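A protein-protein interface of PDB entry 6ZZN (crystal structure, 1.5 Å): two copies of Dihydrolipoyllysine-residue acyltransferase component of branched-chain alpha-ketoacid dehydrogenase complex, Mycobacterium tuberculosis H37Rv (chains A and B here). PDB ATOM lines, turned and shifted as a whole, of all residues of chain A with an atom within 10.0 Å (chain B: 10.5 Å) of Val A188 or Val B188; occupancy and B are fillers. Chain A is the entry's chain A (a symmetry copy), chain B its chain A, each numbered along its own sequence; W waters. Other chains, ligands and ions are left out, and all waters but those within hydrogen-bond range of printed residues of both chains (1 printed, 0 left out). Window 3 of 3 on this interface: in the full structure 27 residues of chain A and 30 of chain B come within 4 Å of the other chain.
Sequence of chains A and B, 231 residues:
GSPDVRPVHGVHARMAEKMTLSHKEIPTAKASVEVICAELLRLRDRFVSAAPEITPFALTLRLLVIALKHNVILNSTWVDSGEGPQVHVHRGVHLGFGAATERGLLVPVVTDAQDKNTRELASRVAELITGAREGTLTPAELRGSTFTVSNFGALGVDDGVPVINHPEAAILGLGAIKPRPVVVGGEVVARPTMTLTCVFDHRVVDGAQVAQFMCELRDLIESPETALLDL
The backbone carbonyl oxygen (O) of Val B182 sits at hydrogen-bond distance from the backbone NH (N) of Val B189 (2.8 Å). N of Arg A180 sits at hydrogen-bond distance from O of Arg A191, at 2.9 Å. O of Thr A193 sits at hydrogen-bond distance from NH1 of Arg A180 (2.8 Å). O of Val A182 lies within hydrogen-bond range of N of Val A189.
Among the printed residues, merely in contact across the chains: Pro A179 with Val B183, Arg A180 with Val B183, Pro A181 with Pro B181, Pro A181 with Val B182, Pro A181 with Val B183, Pro A181 with Val B188, Val A188 with Val B188, Val A189 with Val B188, Ala A190 with Val B183 and Ala A190 with Val B188.
Val A188 touches just one residue of chain B: Val B188. Val B188 touches just these residues of chain A: Pro A181, Val A188, Val A189 and Ala A190. Of chain B, only Pro B181 (3.5 Å), Val B182 (3.6 Å), Val B183 (3.7 Å) and Val B188 (3.9 Å) come within 4 Å of Pro A181. No residue of chain B comes within 4 Å of Gly A186. Val A189 touches just one residue of chain B: Val B188 (3.8 Å). Printed residues of chain B within 4 Å of Arg A180: Val B183 (3.6 Å). Of the printed residues of chain A, Val B183 touches Pro A179, Arg A180, Pro A181 and Ala A190. Pro B179 touches none of the printed residues of chain A. Arg B180 touches none of the printed residues of chain A. The nearest printed residue of chain A that does not touch Pro B181 is Val A188 (5.6 Å).
Of the 15 printed residues of chain A, 6 touch a printed residue of chain B. Hydrophobic or aromatic side chains of chain A within 4 Å of the printed part of chain B: Pro A179, Pro A181, Val A188 and Ala A190. Of the 14 printed residues of chain B, 4 touch a printed residue of chain A.
Arg A180 touches Val B183, but with the chains exchanged Val A183 does not touch Arg B180 (12.0 Å). Pro A181 touches Val B183, but with the chains exchanged Val A183 does not touch Pro B181 (8.5 Å). Val B188 touches its own counterpart, Val A188. Ala A190 touches Val B188, but with the chains exchanged Val A188 does not touch Ala B190 (9.0 Å). Positions printed for both chains: 179, 180, 181, 182, 183, 184, 185, 186, 187, 188, 189, 190 and 191.
Water W1 bridges the backbone carbonyl oxygen of Pro A179 and the backbone NH of Val B183.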
ATOM      1  N   PRO A 179      18.035  18.315 -28.601  1.00  0.00           N
ATOM      2  CA  PRO A 179      19.374  17.817 -28.260  1.00  0.00           C
ATOM      3  C   PRO A 179      19.312  16.642 -27.295  1.00  0.00           C
ATOM      4  O   PRO A 179      18.649  16.697 -26.240  1.00  0.00           O
ATOM      5  CB  PRO A 179      20.035  19.027 -27.577  1.00  0.00           C
ATOM      6  CG  PRO A 179      19.238  20.238 -28.129  1.00  0.00           C
ATOM      7  CD  PRO A 179      17.834  19.707 -28.161  1.00  0.00           C
ATOM      8  N   ARG A 180      20.034  15.576 -27.657  1.00  0.00           N
ATOM      9  CA  ARG A 180      20.148  14.385 -26.818  1.00  0.00           C
ATOM     10  C   ARG A 180      21.578  13.857 -26.916  1.00  0.00           C
ATOM     11  O   ARG A 180      22.276  14.106 -27.912  1.00  0.00           O
ATOM     12  CB  ARG A 180      19.161  13.294 -27.264  1.00  0.00           C
ATOM     13  CG  ARG A 180      17.694  13.733 -27.130  1.00  0.00           C
ATOM     14  CD  ARG A 180      16.764  12.542 -27.318  1.00  0.00           C
ATOM     15  NE  ARG A 180      15.349  12.936 -27.265  1.00  0.00           N
ATOM     16  CZ  ARG A 180      14.678  13.443 -28.298  1.00  0.00           C
ATOM     17  NH1 ARG A 180      15.285  13.632 -29.468  1.00  0.00           N
ATOM     18  NH2 ARG A 180      13.403  13.787 -28.166  1.00  0.00           N
ATOM     19  N   PRO A 181      22.033  13.102 -25.910  1.00  0.00           N
ATOM     20  CA  PRO A 181      23.402  12.551 -25.982  1.00  0.00           C
ATOM     21  C   PRO A 181      23.445  11.356 -26.923  1.00  0.00           C
ATOM     22  O   PRO A 181      22.571  10.489 -26.901  1.00  0.00           O
ATOM     23  CB  PRO A 181      23.678  12.072 -24.544  1.00  0.00           C
ATOM     24  CG  PRO A 181      22.547  12.714 -23.695  1.00  0.00           C
ATOM     25  CD  PRO A 181      21.380  12.786 -24.626  1.00  0.00           C
ATOM     26  N   VAL A 182      24.509  11.299 -27.722  1.00  0.00           N
ATOM     27  CA  VAL A 182      24.767  10.160 -28.611  1.00  0.00           C
ATOM     28  C   VAL A 182      26.292   9.918 -28.624  1.00  0.00           C
ATOM     29  O   VAL A 182      27.064  10.792 -28.200  1.00  0.00           O
ATOM     30  CB  VAL A 182      24.259  10.396 -30.047  1.00  0.00           C
ATOM     31  CG1 VAL A 182      22.732  10.439 -30.113  1.00  0.00           C
ATOM     32  CG2 VAL A 182      24.899  11.641 -30.659  1.00  0.00           C
ATOM     33  N   VAL A 183      26.734   8.746 -29.115  1.00  0.00           N
ATOM     34  CA  VAL A 183      28.165   8.482 -29.256  1.00  0.00           C
ATOM     35  C   VAL A 183      28.543   8.691 -30.719  1.00  0.00           C
ATOM     36  O   VAL A 183      27.946   8.080 -31.611  1.00  0.00           O
ATOM     37  CB  VAL A 183      28.526   7.059 -28.790  1.00  0.00           C
ATOM     38  CG1 VAL A 183      30.000   6.760 -29.072  1.00  0.00           C
ATOM     39  CG2 VAL A 183      28.242   6.902 -27.314  1.00  0.00           C
ATOM     40  N   VAL A 184      29.533   9.559 -30.961  1.00  0.00           N
ATOM     41  CA  VAL A 184      30.056   9.833 -32.303  1.00  0.00           C
ATOM     42  C   VAL A 184      31.568   9.699 -32.199  1.00  0.00           C
ATOM     43  O   VAL A 184      32.200  10.351 -31.363  1.00  0.00           O
ATOM     44  CB  VAL A 184      29.654  11.239 -32.805  1.00  0.00           C
ATOM     45  CG1 VAL A 184      30.357  11.573 -34.131  1.00  0.00           C
ATOM     46  CG2 VAL A 184      28.137  11.356 -32.941  1.00  0.00           C
ATOM     47  N   GLY A 185      32.128   8.783 -32.976  1.00  0.00           N
ATOM     48  CA  GLY A 185      33.569   8.546 -32.949  1.00  0.00           C
ATOM     49  C   GLY A 185      34.113   8.183 -31.580  1.00  0.00           C
ATOM     50  O   GLY A 185      35.174   8.671 -31.171  1.00  0.00           O
ATOM     51  N   GLY A 186      33.339   7.394 -30.831  1.00  0.00           N
ATOM     52  CA  GLY A 186      33.738   6.969 -29.502  1.00  0.00           C
ATOM     53  C   GLY A 186      33.555   7.989 -28.391  1.00  0.00           C
ATOM     54  O   GLY A 186      33.861   7.695 -27.234  1.00  0.00           O
ATOM     55  N   GLU A 187      33.078   9.191 -28.724  1.00  0.00           N
ATOM     56  CA  GLU A 187      32.882  10.245 -27.732  1.00  0.00           C
ATOM     57  C   GLU A 187      31.400  10.533 -27.512  1.00  0.00           C
ATOM     58  O   GLU A 187      30.629  10.514 -28.471  1.00  0.00           O
ATOM     59  CB  GLU A 187      33.539  11.553 -28.216  1.00  0.00           C
ATOM     60  CG  GLU A 187      35.028  11.427 -28.496  1.00  0.00           C
ATOM     61  CD  GLU A 187      35.892  11.156 -27.280  1.00  0.00           C
ATOM     62  OE1 GLU A 187      35.484  11.525 -26.155  1.00  0.00           O
ATOM     63  OE2 GLU A 187      36.993  10.586 -27.457  1.00  0.00           O
ATOM     64  N   VAL A 188      31.018  10.828 -26.261  1.00  0.00           N
ATOM     65  CA  VAL A 188      29.635  11.196 -25.976  1.00  0.00           C
ATOM     66  C   VAL A 188      29.505  12.667 -26.312  1.00  0.00           C
ATOM     67  O   VAL A 188      30.275  13.500 -25.804  1.00  0.00           O
ATOM     68  CB  VAL A 188      29.230  10.942 -24.519  1.00  0.00           C
ATOM     69  CG1 VAL A 188      27.809  11.452 -24.279  1.00  0.00           C
ATOM     70  CG2 VAL A 188      29.331   9.454 -24.195  1.00  0.00           C
ATOM     71  N   VAL A 189      28.549  12.990 -27.189  1.00  0.00           N
ATOM     72  CA  VAL A 189      28.341  14.379 -27.614  1.00  0.00           C
ATOM     73  C   VAL A 189      26.852  14.701 -27.629  1.00  0.00           C
ATOM     74  O   VAL A 189      26.010  13.789 -27.625  1.00  0.00           O
ATOM     75  CB  VAL A 189      28.946  14.600 -29.032  1.00  0.00           C
ATOM     76  CG1 VAL A 189      30.463  14.399 -29.022  1.00  0.00           C
ATOM     77  CG2 VAL A 189      28.291  13.683 -30.060  1.00  0.00           C
ATOM     78  N   ALA A 190      26.522  15.993 -27.706  1.00  0.00           N
ATOM     79  CA  ALA A 190      25.140  16.409 -27.837  1.00  0.00           C
ATOM     80  C   ALA A 190      24.830  16.610 -29.315  1.00  0.00           C
ATOM     81  O   ALA A 190      25.606  17.243 -30.046  1.00  0.00           O
ATOM     82  CB  ALA A 190      24.932  17.724 -27.108  1.00  0.00           C
ATOM     83  N   ARG A 191      23.682  16.111 -29.754  1.00  0.00           N
ATOM     84  CA  ARG A 191      23.237  16.349 -31.127  1.00  0.00           C
ATOM     85  C   ARG A 191      21.736  16.492 -31.102  1.00  0.00           C
ATOM     86  O   ARG A 191      21.070  15.768 -30.347  1.00  0.00           O
ATOM     87  CB  ARG A 191      23.519  15.121 -32.027  1.00  0.00           C
ATOM     88  CG  ARG A 191      24.988  14.840 -32.320  1.00  0.00           C
ATOM     89  CD  ARG A 191      25.558  15.811 -33.346  1.00  0.00           C
ATOM     90  NE  ARG A 191      26.961  15.503 -33.654  1.00  0.00           N
ATOM     91  CZ  ARG A 191      27.999  15.972 -32.967  1.00  0.00           C
ATOM     92  NH1 ARG A 191      27.807  16.747 -31.905  1.00  0.00           N
ATOM     93  NH2 ARG A 191      29.244  15.687 -33.349  1.00  0.00           N
ATOM     94  N   PRO A 192      21.146  17.282 -32.012  1.00  0.00           N
ATOM     95  CA  PRO A 192      19.681  17.188 -32.198  1.00  0.00           C
ATOM     96  C   PRO A 192      19.397  15.799 -32.753  1.00  0.00           C
ATOM     97  O   PRO A 192      20.114  15.325 -33.646  1.00  0.00           O
ATOM     98  CB  PRO A 192      19.368  18.224 -33.302  1.00  0.00           C
ATOM     99  CG  PRO A 192      20.648  18.942 -33.561  1.00  0.00           C
ATOM    100  CD  PRO A 192      21.792  18.149 -33.015  1.00  0.00           C
ATOM    101  N   THR A 193      18.420  15.107 -32.174  1.00  0.00           N
ATOM    102  CA  THR A 193      18.070  13.768 -32.658  1.00  0.00           C
ATOM    103  C   THR A 193      16.551  13.616 -32.674  1.00  0.00           C
ATOM    104  O   THR A 193      15.837  14.413 -32.069  1.00  0.00           O
ATOM    105  CB  THR A 193      18.653  12.649 -31.719  1.00  0.00           C
ATOM    106  OG1 THR A 193      17.917  12.647 -30.484  1.00  0.00           O
ATOM    107  CG2 THR A 193      20.139  12.790 -31.448  1.00  0.00           C
ATOM    108  N   ILE B  36      13.008  14.581 -16.438  1.00  0.00           N
ATOM    109  CA  ILE B  36      14.123  14.713 -15.495  1.00  0.00           C
ATOM    110  C   ILE B  36      13.540  14.738 -14.069  1.00  0.00           C
ATOM    111  O   ILE B  36      12.602  15.489 -13.779  1.00  0.00           O
ATOM    112  CB  ILE B  36      14.960  15.960 -15.820  1.00  0.00           C
ATOM    113  CG1 ILE B  36      15.666  15.757 -17.184  1.00  0.00           C
ATOM    114  CG2 ILE B  36      15.985  16.231 -14.713  1.00  0.00           C
ATOM    115  CD1 ILE B  36      16.277  17.054 -17.730  1.00  0.00           C
ATOM    116  N   PRO B 179      19.780   7.249 -12.870  1.00  0.00           N
ATOM    117  CA  PRO B 179      20.625   8.201 -13.603  1.00  0.00           C
ATOM    118  C   PRO B 179      20.796   7.802 -15.062  1.00  0.00           C
ATOM    119  O   PRO B 179      21.154   6.652 -15.386  1.00  0.00           O
ATOM    120  CB  PRO B 179      21.974   8.111 -12.869  1.00  0.00           C
ATOM    121  CG  PRO B 179      21.589   7.584 -11.463  1.00  0.00           C
ATOM    122  CD  PRO B 179      20.516   6.583 -11.780  1.00  0.00           C
ATOM    123  N   ARG B 180      20.557   8.777 -15.946  1.00  0.00           N
ATOM    124  CA  ARG B 180      20.739   8.592 -17.384  1.00  0.00           C
ATOM    125  C   ARG B 180      21.321   9.878 -17.967  1.00  0.00           C
ATOM    126  O   ARG B 180      21.145  10.966 -17.398  1.00  0.00           O
ATOM    127  CB  ARG B 180      19.407   8.265 -18.076  1.00  0.00           C
ATOM    128  CG  ARG B 180      18.793   6.944 -17.583  1.00  0.00           C
ATOM    129  CD  ARG B 180      17.634   6.530 -18.480  1.00  0.00           C
ATOM    130  NE  ARG B 180      16.977   5.306 -18.000  1.00  0.00           N
ATOM    131  CZ  ARG B 180      16.055   5.284 -17.038  1.00  0.00           C
ATOM    132  NH1 ARG B 180      15.680   6.412 -16.438  1.00  0.00           N
ATOM    133  NH2 ARG B 180      15.519   4.135 -16.649  1.00  0.00           N
ATOM    134  N   PRO B 181      21.996   9.788 -19.119  1.00  0.00           N
ATOM    135  CA  PRO B 181      22.550  11.016 -19.729  1.00  0.00           C
ATOM    136  C   PRO B 181      21.450  11.812 -20.414  1.00  0.00           C
ATOM    137  O   PRO B 181      20.598  11.261 -21.113  1.00  0.00           O
ATOM    138  CB  PRO B 181      23.528  10.484 -20.794  1.00  0.00           C
ATOM    139  CG  PRO B 181      23.693   8.977 -20.454  1.00  0.00           C
ATOM    140  CD  PRO B 181      22.373   8.581 -19.876  1.00  0.00           C
ATOM    141  N   VAL B 182      21.509  13.131 -20.242  1.00  0.00           N
ATOM    142  CA  VAL B 182      20.596  14.057 -20.921  1.00  0.00           C
ATOM    143  C   VAL B 182      21.406  15.318 -21.293  1.00  0.00           C
ATOM    144  O   VAL B 182      22.509  15.526 -20.765  1.00  0.00           O
ATOM    145  CB  VAL B 182      19.385  14.447 -20.051  1.00  0.00           C
ATOM    146  CG1 VAL B 182      18.439  13.267 -19.824  1.00  0.00           C
ATOM    147  CG2 VAL B 182      19.834  15.088 -18.738  1.00  0.00           C
ATOM    148  N   VAL B 183      20.868  16.164 -22.189  1.00  0.00           N
ATOM    149  CA  VAL B 183      21.524  17.429 -22.518  1.00  0.00           C
ATOM    150  C   VAL B 183      20.814  18.543 -21.754  1.00  0.00           C
ATOM    151  O   VAL B 183      19.594  18.698 -21.867  1.00  0.00           O
ATOM    152  CB  VAL B 183      21.503  17.699 -24.033  1.00  0.00           C
ATOM    153  CG1 VAL B 183      22.074  19.086 -24.339  1.00  0.00           C
ATOM    154  CG2 VAL B 183      22.298  16.643 -24.766  1.00  0.00           C
ATOM    155  N   VAL B 184      21.583  19.313 -20.973  1.00  0.00           N
ATOM    156  CA  VAL B 184      21.071  20.459 -20.216  1.00  0.00           C
ATOM    157  C   VAL B 184      21.997  21.622 -20.539  1.00  0.00           C
ATOM    158  O   VAL B 184      23.215  21.520 -20.370  1.00  0.00           O
ATOM    159  CB  VAL B 184      21.035  20.180 -18.696  1.00  0.00           C
ATOM    160  CG1 VAL B 184      20.665  21.450 -17.911  1.00  0.00           C
ATOM    161  CG2 VAL B 184      20.076  19.036 -18.375  1.00  0.00           C
ATOM    162  N   GLY B 185      21.431  22.683 -21.097  1.00  0.00           N
ATOM    163  CA  GLY B 185      22.221  23.852 -21.472  1.00  0.00           C
ATOM    164  C   GLY B 185      23.357  23.553 -22.433  1.00  0.00           C
ATOM    165  O   GLY B 185      24.471  24.069 -22.276  1.00  0.00           O
ATOM    166  N   GLY B 186      23.103  22.644 -23.377  1.00  0.00           N
ATOM    167  CA  GLY B 186      24.100  22.263 -24.361  1.00  0.00           C
ATOM    168  C   GLY B 186      25.165  21.289 -23.890  1.00  0.00           C
ATOM    169  O   GLY B 186      26.038  20.911 -24.673  1.00  0.00           O
ATOM    170  N   GLU B 187      25.122  20.889 -22.616  1.00  0.00           N
ATOM    171  CA  GLU B 187      26.110  19.967 -22.063  1.00  0.00           C
ATOM    172  C   GLU B 187      25.488  18.612 -21.741  1.00  0.00           C
ATOM    173  O   GLU B 187      24.350  18.562 -21.274  1.00  0.00           O
ATOM    174  CB  GLU B 187      26.684  20.535 -20.750  1.00  0.00           C
ATOM    175  CG  GLU B 187      27.332  21.901 -20.902  1.00  0.00           C
ATOM    176  CD  GLU B 187      28.590  21.928 -21.747  1.00  0.00           C
ATOM    177  OE1 GLU B 187      29.274  20.883 -21.846  1.00  0.00           O
ATOM    178  OE2 GLU B 187      28.903  23.006 -22.302  1.00  0.00           O
ATOM    179  N   VAL B 188      26.246  17.528 -21.961  1.00  0.00           N
ATOM    180  CA  VAL B 188      25.759  16.199 -21.604  1.00  0.00           C
ATOM    181  C   VAL B 188      26.027  16.027 -20.124  1.00  0.00           C
ATOM    182  O   VAL B 188      27.172  16.193 -19.668  1.00  0.00           O
ATOM    183  CB  VAL B 188      26.431  15.075 -22.404  1.00  0.00           C
ATOM    184  CG1 VAL B 188      25.946  13.717 -21.896  1.00  0.00           C
ATOM    185  CG2 VAL B 188      26.129  15.234 -23.891  1.00  0.00           C
ATOM    186  N   VAL B 189      24.971  15.722 -19.364  1.00  0.00           N
ATOM    187  CA  VAL B 189      25.098  15.555 -17.912  1.00  0.00           C
ATOM    188  C   VAL B 189      24.321  14.325 -17.460  1.00  0.00           C
ATOM    189  O   VAL B 189      23.460  13.818 -18.195  1.00  0.00           O
ATOM    190  CB  VAL B 189      24.562  16.820 -17.180  1.00  0.00           C
ATOM    191  CG1 VAL B 189      25.399  18.053 -17.524  1.00  0.00           C
ATOM    192  CG2 VAL B 189      23.091  17.063 -17.505  1.00  0.00           C
ATOM    193  N   ALA B 190      24.579  13.876 -16.228  1.00  0.00           N
ATOM    194  CA  ALA B 190      23.823  12.781 -15.654  1.00  0.00           C
ATOM    195  C   ALA B 190      22.688  13.359 -14.818  1.00  0.00           C
ATOM    196  O   ALA B 190      22.895  14.287 -14.022  1.00  0.00           O
ATOM    197  CB  ALA B 190      24.725  11.956 -14.754  1.00  0.00           C
ATOM    198  N   ARG B 191      21.497  12.794 -14.964  1.00  0.00           N
ATOM    199  CA  ARG B 191      20.368  13.197 -14.125  1.00  0.00           C
ATOM    200  C   ARG B 191      19.541  11.967 -13.849  1.00  0.00           C
ATOM    201  O   ARG B 191      19.382  11.129 -14.750  1.00  0.00           O
ATOM    202  CB  ARG B 191      19.427  14.165 -14.883  1.00  0.00           C
ATOM    203  CG  ARG B 191      19.994  15.551 -15.167  1.00  0.00           C
ATOM    204  CD  ARG B 191      20.004  16.426 -13.919  1.00  0.00           C
ATOM    205  NE  ARG B 191      20.510  17.774 -14.215  1.00  0.00           N
ATOM    206  CZ  ARG B 191      21.796  18.113 -14.189  1.00  0.00           C
ATOM    207  NH1 ARG B 191      22.726  17.204 -13.918  1.00  0.00           N
ATOM    208  NH2 ARG B 191      22.165  19.374 -14.416  1.00  0.00           N
HETATM  209  O   HOH W   1      18.532  15.354 -23.706  1.00  0.00           O
